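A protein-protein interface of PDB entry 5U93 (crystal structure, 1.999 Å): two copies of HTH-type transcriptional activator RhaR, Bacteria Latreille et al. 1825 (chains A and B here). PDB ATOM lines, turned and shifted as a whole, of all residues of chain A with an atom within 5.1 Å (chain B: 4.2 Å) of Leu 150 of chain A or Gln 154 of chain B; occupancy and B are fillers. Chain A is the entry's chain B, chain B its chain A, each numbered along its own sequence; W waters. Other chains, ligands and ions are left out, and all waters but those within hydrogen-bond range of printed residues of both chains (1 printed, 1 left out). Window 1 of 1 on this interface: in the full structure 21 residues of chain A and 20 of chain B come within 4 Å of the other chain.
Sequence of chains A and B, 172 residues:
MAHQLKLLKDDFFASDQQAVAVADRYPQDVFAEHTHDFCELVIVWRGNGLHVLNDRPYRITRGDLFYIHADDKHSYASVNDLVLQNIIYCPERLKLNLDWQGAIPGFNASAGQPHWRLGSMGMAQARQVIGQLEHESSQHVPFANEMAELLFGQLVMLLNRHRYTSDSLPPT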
ATOM      1  N   LEU A  96      -5.007 -16.684  20.422  1.00  0.00           N
ATOM      2  CA  LEU A  96      -4.798 -15.273  20.124  1.00  0.00           C
ATOM      3  C   LEU A  96      -4.563 -14.500  21.425  1.00  0.00           C
ATOM      4  O   LEU A  96      -5.233 -14.756  22.430  1.00  0.00           O
ATOM      5  CB  LEU A  96      -6.025 -14.735  19.380  1.00  0.00           C
ATOM      6  CG  LEU A  96      -5.892 -13.458  18.560  1.00  0.00           C
ATOM      7  CD1 LEU A  96      -4.898 -13.661  17.418  1.00  0.00           C
ATOM      8  CD2 LEU A  96      -7.269 -13.081  18.023  1.00  0.00           C
ATOM      9  N   GLN A 132     -20.502 -15.496   9.946  1.00  0.00           N
ATOM     10  CA  GLN A 132     -19.147 -15.782   9.461  1.00  0.00           C
ATOM     11  C   GLN A 132     -18.441 -16.795  10.364  1.00  0.00           C
ATOM     12  O   GLN A 132     -17.767 -17.713   9.881  1.00  0.00           O
ATOM     13  CB  GLN A 132     -18.307 -14.494   9.379  1.00  0.00           C
ATOM     14  CG  GLN A 132     -18.868 -13.418   8.439  1.00  0.00           C
ATOM     15  CD  GLN A 132     -18.141 -12.078   8.572  1.00  0.00           C
ATOM     16  OE1 GLN A 132     -16.912 -12.017   8.511  1.00  0.00           O
ATOM     17  NE2 GLN A 132     -18.904 -11.002   8.747  1.00  0.00           N
ATOM     18  N   GLU A 146      -7.605 -19.922  12.688  1.00  0.00           N
ATOM     19  CA  GLU A 146      -7.220 -18.539  12.911  1.00  0.00           C
ATOM     20  C   GLU A 146      -8.389 -17.584  12.667  1.00  0.00           C
ATOM     21  O   GLU A 146      -8.620 -16.672  13.464  1.00  0.00           O
ATOM     22  CB  GLU A 146      -6.034 -18.141  12.018  1.00  0.00           C
ATOM     23  CG  GLU A 146      -4.713 -18.854  12.328  1.00  0.00           C
ATOM     24  CD  GLU A 146      -4.547 -20.191  11.593  1.00  0.00           C
ATOM     25  OE1 GLU A 146      -5.545 -20.778  11.122  1.00  0.00           O
ATOM     26  OE2 GLU A 146      -3.404 -20.657  11.488  1.00  0.00           O
ATOM     27  N   MET A 147      -9.108 -17.780  11.561  1.00  0.00           N
ATOM     28  CA  MET A 147     -10.269 -16.935  11.243  1.00  0.00           C
ATOM     29  C   MET A 147     -11.332 -17.028  12.329  1.00  0.00           C
ATOM     30  O   MET A 147     -11.920 -16.014  12.703  1.00  0.00           O
ATOM     31  CB  MET A 147     -10.882 -17.313   9.881  1.00  0.00           C
ATOM     32  CG  MET A 147     -10.047 -16.871   8.686  1.00  0.00           C
ATOM     33  SD  MET A 147     -10.103 -14.913   8.499  1.00  0.00           S
ATOM     34  CE  MET A 147     -12.006 -14.692   8.255  1.00  0.00           C
ATOM     35  N   ALA A 148     -11.601 -18.241  12.816  1.00  0.00           N
ATOM     36  CA  ALA A 148     -12.616 -18.406  13.867  1.00  0.00           C
ATOM     37  C   ALA A 148     -12.253 -17.601  15.121  1.00  0.00           C
ATOM     38  O   ALA A 148     -13.111 -16.928  15.698  1.00  0.00           O
ATOM     39  CB  ALA A 148     -12.830 -19.902  14.214  1.00  0.00           C
ATOM     40  N   GLU A 149     -10.986 -17.665  15.540  1.00  0.00           N
ATOM     41  CA  GLU A 149     -10.533 -16.890  16.690  1.00  0.00           C
ATOM     42  C   GLU A 149     -10.625 -15.392  16.445  1.00  0.00           C
ATOM     43  O   GLU A 149     -11.016 -14.632  17.340  1.00  0.00           O
ATOM     44  CB  GLU A 149      -9.090 -17.262  17.093  1.00  0.00           C
ATOM     45  CG  GLU A 149      -8.977 -18.607  17.782  1.00  0.00           C
ATOM     46  CD  GLU A 149      -7.912 -18.630  18.876  1.00  0.00           C
ATOM     47  OE1 GLU A 149      -7.417 -19.731  19.198  1.00  0.00           O
ATOM     48  OE2 GLU A 149      -7.588 -17.551  19.427  1.00  0.00           O
ATOM     49  N   LEU A 150     -10.239 -14.956  15.245  1.00  0.00           N
ATOM     50  CA  LEU A 150     -10.303 -13.532  14.921  1.00  0.00           C
ATOM     51  C   LEU A 150     -11.742 -13.030  14.918  1.00  0.00           C
ATOM     52  O   LEU A 150     -12.022 -11.920  15.371  1.00  0.00           O
ATOM     53  CB  LEU A 150      -9.639 -13.255  13.569  1.00  0.00           C
ATOM     54  CG  LEU A 150      -8.120 -13.455  13.540  1.00  0.00           C
ATOM     55  CD1 LEU A 150      -7.607 -13.639  12.088  1.00  0.00           C
ATOM     56  CD2 LEU A 150      -7.422 -12.264  14.221  1.00  0.00           C
ATOM     57  N   LEU A 151     -12.645 -13.853  14.398  1.00  0.00           N
ATOM     58  CA  LEU A 151     -14.067 -13.521  14.350  1.00  0.00           C
ATOM     59  C   LEU A 151     -14.700 -13.552  15.746  1.00  0.00           C
ATOM     60  O   LEU A 151     -15.509 -12.693  16.087  1.00  0.00           O
ATOM     61  CB  LEU A 151     -14.798 -14.483  13.404  1.00  0.00           C
ATOM     62  CG  LEU A 151     -14.601 -14.199  11.905  1.00  0.00           C
ATOM     63  CD1 LEU A 151     -14.980 -15.438  11.099  1.00  0.00           C
ATOM     64  CD2 LEU A 151     -15.446 -12.987  11.448  1.00  0.00           C
ATOM     65  N   PHE A 152     -14.316 -14.535  16.556  1.00  0.00           N
ATOM     66  CA  PHE A 152     -14.774 -14.592  17.946  1.00  0.00           C
ATOM     67  C   PHE A 152     -14.307 -13.351  18.705  1.00  0.00           C
ATOM     68  O   PHE A 152     -15.077 -12.744  19.469  1.00  0.00           O
ATOM     69  CB  PHE A 152     -14.258 -15.863  18.627  1.00  0.00           C
ATOM     70  CG  PHE A 152     -14.759 -16.051  20.039  1.00  0.00           C
ATOM     71  CD1 PHE A 152     -16.119 -16.021  20.312  1.00  0.00           C
ATOM     72  CD2 PHE A 152     -13.876 -16.301  21.078  1.00  0.00           C
ATOM     73  CE1 PHE A 152     -16.598 -16.209  21.603  1.00  0.00           C
ATOM     74  CE2 PHE A 152     -14.348 -16.484  22.380  1.00  0.00           C
ATOM     75  CZ  PHE A 152     -15.714 -16.442  22.632  1.00  0.00           C
ATOM     76  N   GLY A 153     -13.045 -12.968  18.484  1.00  0.00           N
ATOM     77  CA  GLY A 153     -12.524 -11.733  19.046  1.00  0.00           C
ATOM     78  C   GLY A 153     -13.330 -10.507  18.624  1.00  0.00           C
ATOM     79  O   GLY A 153     -13.642  -9.633  19.435  1.00  0.00           O
ATOM     80  N   GLN A 154     -13.668 -10.426  17.343  1.00  0.00           N
ATOM     81  CA  GLN A 154     -14.488  -9.314  16.876  1.00  0.00           C
ATOM     82  C   GLN A 154     -15.873  -9.339  17.535  1.00  0.00           C
ATOM     83  O   GLN A 154     -16.419  -8.294  17.914  1.00  0.00           O
ATOM     84  CB  GLN A 154     -14.620  -9.354  15.350  1.00  0.00           C
ATOM     85  CG  GLN A 154     -15.526  -8.261  14.770  1.00  0.00           C
ATOM     86  CD  GLN A 154     -15.737  -8.416  13.263  1.00  0.00           C
ATOM     87  OE1 GLN A 154     -15.260  -9.372  12.644  1.00  0.00           O
ATOM     88  NE2 GLN A 154     -16.456  -7.474  12.670  1.00  0.00           N
ATOM     89  N   LEU B  98      -0.414 -12.883  15.414  1.00  0.00           N
ATOM     90  CA  LEU B  98      -0.479 -13.630  14.147  1.00  0.00           C
ATOM     91  C   LEU B  98       0.908 -13.598  13.540  1.00  0.00           C
ATOM     92  O   LEU B  98       1.705 -12.706  13.861  1.00  0.00           O
ATOM     93  CB  LEU B  98      -1.443 -12.969  13.160  1.00  0.00           C
ATOM     94  CG  LEU B  98      -2.920 -12.941  13.546  1.00  0.00           C
ATOM     95  CD1 LEU B  98      -3.688 -12.271  12.414  1.00  0.00           C
ATOM     96  CD2 LEU B  98      -3.450 -14.347  13.816  1.00  0.00           C
ATOM     97  N   VAL B 129     -14.578  -7.420   4.599  1.00  0.00           N
ATOM     98  CA  VAL B 129     -13.697  -7.097   5.720  1.00  0.00           C
ATOM     99  C   VAL B 129     -13.200  -5.654   5.654  1.00  0.00           C
ATOM    100  O   VAL B 129     -13.145  -4.948   6.659  1.00  0.00           O
ATOM    101  CB  VAL B 129     -12.495  -8.067   5.802  1.00  0.00           C
ATOM    102  CG1 VAL B 129     -11.541  -7.643   6.906  1.00  0.00           C
ATOM    103  CG2 VAL B 129     -12.995  -9.452   6.095  1.00  0.00           C
ATOM    104  N   LEU B 150      -7.909  -6.575  14.553  1.00  0.00           N
ATOM    105  CA  LEU B 150      -8.539  -7.885  14.348  1.00  0.00           C
ATOM    106  C   LEU B 150      -9.042  -8.020  12.912  1.00  0.00           C
ATOM    107  O   LEU B 150      -8.892  -9.073  12.288  1.00  0.00           O
ATOM    108  CB  LEU B 150      -9.714  -8.106  15.307  1.00  0.00           C
ATOM    109  CG  LEU B 150      -9.464  -8.329  16.801  1.00  0.00           C
ATOM    110  CD1 LEU B 150     -10.744  -8.120  17.581  1.00  0.00           C
ATOM    111  CD2 LEU B 150      -8.944  -9.733  17.051  1.00  0.00           C
ATOM    112  N   LEU B 151      -9.669  -6.969  12.398  1.00  0.00           N
ATOM    113  CA  LEU B 151     -10.144  -6.976  11.007  1.00  0.00           C
ATOM    114  C   LEU B 151      -8.996  -7.029   9.995  1.00  0.00           C
ATOM    115  O   LEU B 151      -9.090  -7.711   8.965  1.00  0.00           O
ATOM    116  CB  LEU B 151     -11.025  -5.741  10.738  1.00  0.00           C
ATOM    117  CG  LEU B 151     -12.380  -5.779  11.456  1.00  0.00           C
ATOM    118  CD1 LEU B 151     -12.987  -4.387  11.520  1.00  0.00           C
ATOM    119  CD2 LEU B 151     -13.325  -6.770  10.745  1.00  0.00           C
ATOM    120  N   PHE B 152      -7.915  -6.301  10.273  1.00  0.00           N
ATOM    121  CA  PHE B 152      -6.725  -6.383   9.421  1.00  0.00           C
ATOM    122  C   PHE B 152      -6.171  -7.816   9.434  1.00  0.00           C
ATOM    123  O   PHE B 152      -5.772  -8.369   8.396  1.00  0.00           O
ATOM    124  CB  PHE B 152      -5.656  -5.387   9.893  1.00  0.00           C
ATOM    125  CG  PHE B 152      -4.396  -5.393   9.047  1.00  0.00           C
ATOM    126  CD1 PHE B 152      -4.435  -5.010   7.712  1.00  0.00           C
ATOM    127  CD2 PHE B 152      -3.176  -5.769   9.596  1.00  0.00           C
ATOM    128  CE1 PHE B 152      -3.272  -5.012   6.921  1.00  0.00           C
ATOM    129  CE2 PHE B 152      -2.005  -5.771   8.812  1.00  0.00           C
ATOM    130  CZ  PHE B 152      -2.063  -5.390   7.471  1.00  0.00           C
ATOM    131  N   GLY B 153      -6.156  -8.428  10.608  1.00  0.00           N
ATOM    132  CA  GLY B 153      -5.760  -9.819  10.711  1.00  0.00           C
ATOM    133  C   GLY B 153      -6.637 -10.730   9.847  1.00  0.00           C
ATOM    134  O   GLY B 153      -6.133 -11.611   9.156  1.00  0.00           O
ATOM    135  N   GLN B 154      -7.950 -10.524   9.891  1.00  0.00           N
ATOM    136  CA  GLN B 154      -8.871 -11.294   9.043  1.00  0.00           C
ATOM    137  C   GLN B 154      -8.550 -11.068   7.553  1.00  0.00           C
ATOM    138  O   GLN B 154      -8.534 -12.003   6.761  1.00  0.00           O
ATOM    139  CB  GLN B 154     -10.312 -10.882   9.319  1.00  0.00           C
ATOM    140  CG  GLN B 154     -10.860 -11.264  10.714  1.00  0.00           C
ATOM    141  CD  GLN B 154     -12.303 -10.821  10.886  1.00  0.00           C
ATOM    142  OE1 GLN B 154     -13.037 -10.721   9.903  1.00  0.00           O
ATOM    143  NE2 GLN B 154     -12.715 -10.536  12.129  1.00  0.00           N
ATOM    144  N   LEU B 155      -8.295  -9.822   7.181  1.00  0.00           N
ATOM    145  CA  LEU B 155      -8.000  -9.504   5.787  1.00  0.00           C
ATOM    146  C   LEU B 155      -6.735 -10.219   5.349  1.00  0.00           C
ATOM    147  O   LEU B 155      -6.684 -10.801   4.279  1.00  0.00           O
ATOM    148  CB  LEU B 155      -7.767  -8.010   5.629  1.00  0.00           C
ATOM    149  CG  LEU B 155      -8.050  -7.219   4.343  1.00  0.00           C
ATOM    150  CD1 LEU B 155      -7.023  -6.068   4.092  1.00  0.00           C
ATOM    151  CD2 LEU B 155      -8.295  -8.055   3.112  1.00  0.00           C
ATOM    152  N   VAL B 156      -5.691 -10.123   6.162  1.00  0.00           N
ATOM    153  CA  VAL B 156      -4.407 -10.760   5.844  1.00  0.00           C
ATOM    154  C   VAL B 156      -4.522 -12.294   5.677  1.00  0.00           C
ATOM    155  O   VAL B 156      -3.939 -12.859   4.747  1.00  0.00           O
ATOM    156  CB  VAL B 156      -3.324 -10.355   6.890  1.00  0.00           C
ATOM    157  CG1 VAL B 156      -2.122 -11.269   6.825  1.00  0.00           C
ATOM    158  CG2 VAL B 156      -2.914  -8.865   6.701  1.00  0.00           C
ATOM    159  N   MET B 157      -5.269 -12.963   6.562  1.00  0.00           N
ATOM    160  CA  MET B 157      -5.505 -14.406   6.444  1.00  0.00           C
ATOM    161  C   MET B 157      -6.307 -14.739   5.184  1.00  0.00           C
ATOM    162  O   MET B 157      -6.011 -15.703   4.489  1.00  0.00           O
ATOM    163  CB  MET B 157      -6.290 -14.976   7.649  1.00  0.00           C
ATOM    164  CG  MET B 157      -5.668 -14.828   9.023  1.00  0.00           C
ATOM    165  SD  MET B 157      -4.112 -16.004   9.266  1.00  0.00           S
ATOM    166  CE  MET B 157      -2.840 -14.738   8.739  1.00  0.00           C
ATOM    167  N   LEU B 158      -7.351 -13.964   4.919  1.00  0.00           N
ATOM    168  CA  LEU B 158      -8.203 -14.213   3.746  1.00  0.00           C
ATOM    169  C   LEU B 158      -7.423 -14.023   2.460  1.00  0.00           C
ATOM    170  O   LEU B 158      -7.593 -14.791   1.515  1.00  0.00           O
ATOM    171  CB  LEU B 158      -9.403 -13.253   3.738  1.00  0.00           C
ATOM    172  CG  LEU B 158     -10.497 -13.588   4.735  1.00  0.00           C
ATOM    173  CD1 LEU B 158     -11.438 -12.390   4.810  1.00  0.00           C
ATOM    174  CD2 LEU B 158     -11.236 -14.858   4.291  1.00  0.00           C
HETATM  175  O   HOH W   1     -14.013 -11.991   7.635  1.00  0.00           O
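Hydrophobic or aromatic side chains of chain B that line the printed part of chain A: Leu 98, Leu 150, Leu 151, Met 157 and Leu 158. Printed residues of chain A that touch a printed residue of chain B: Leu 96, Glu 146, Met 147, Leu 150, Leu 151, Gly 153 and Gln 154. Among the printed residues, 14 pairs touch across the chains.
Leu 96 of chain A touches Leu 98 of chain B. Leu 150 of chain B touches Leu 96 of chain A. Glu 146 of chain A touches Met 157 of chain B. CE of Met 147 of chain A touches CG of Leu 158 of chain B (3.99 Å). CD1 of Leu 150 of chain A touches C of Gly 153 of chain B (3.8 Å). O of Leu 150 of chain A touches NE2 of Gln 154 of chain B (3.6 Å). Leu 150 of chain A touches Met 157 of chain B (CD1 to CG, 3.8 Å). Leu 150 of chain B touches Gly 153 of chain A (CD1 to C, 3.7 Å). Leu 150 of chain B touches Gln 154 of chain A (CD1 to N, 3.7 Å). CD2 of Leu 151 of chain B touches NE2 of Gln 154 of chain A, 3.7 Å away.
NE2 of Gln 154 of chain B is in hydrogen-bond range of OE1 of Gln 154 of chain A (2.8 Å). The side-chain sulfur of Met 147 of chain A sits close to the backbone carbonyl oxygen of Gln 154 of chain B (3.7 Å).
Leu 150 of chain A touches Gly 153 of chain B, and with the chains exchanged Gly 153 of chain A touches Leu 150 of chain B. Leu 150 of chain A touches Gln 154 of chain B, and with the chains exchanged Gln 154 of chain A touches Leu 150 of chain B. Leu 151 of chain A touches Gln 154 of chain B, and with the chains exchanged Gln 154 of chain A touches Leu 151 of chain B. Gln 154 of chain A touches its own counterpart, Gln 154 of chain B. Positions printed for both chains: 150, 151, 152, 153 and 154. Of the 14 pairs that touch across the chains among the printed residues, 7 have their exchanged pair printed and touching as well.
N of Leu 96 of chain A is in hydrogen-bond range of OE2 of Glu 149 of chain A (2.9 Å).
Water W1 lies within hydrogen-bond range of the side-chain amide oxygen of Gln 154 of chain B (2.8 Å) and the side-chain amide oxygen of Gln 132 of chain A (3.0 Å).
Ala 148 of chain A touches none of the printed residues of chain B. Printed residues of chain B within 4 Å of Leu 150 of chain A: Gly 153 (3.8 Å), Gln 154 (3.6 Å) and Met 157 (3.8 Å). Of the printed residues of chain A, Leu 98 of chain B touches Leu 96 (3.9 Å). Printed residues of chain A within 4 Å of Leu 151 of chain B: Gln 154 (3.7 Å). Phe 152 of chain B touches none of the printed residues of chain A. Of chain A, only Met 147 (3.7 Å), Leu 150 (3.6 Å), Leu 151 (3.7 Å) and Gln 154 (2.8 Å) come within 4 Å of Gln 154 of chain B. Of the printed residues of chain A, Leu 158 of chain B touches Met 147. The nearest printed residue of chain A that does not touch Leu 150 of chain B is Leu 150 of chain A (4.01 Å).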
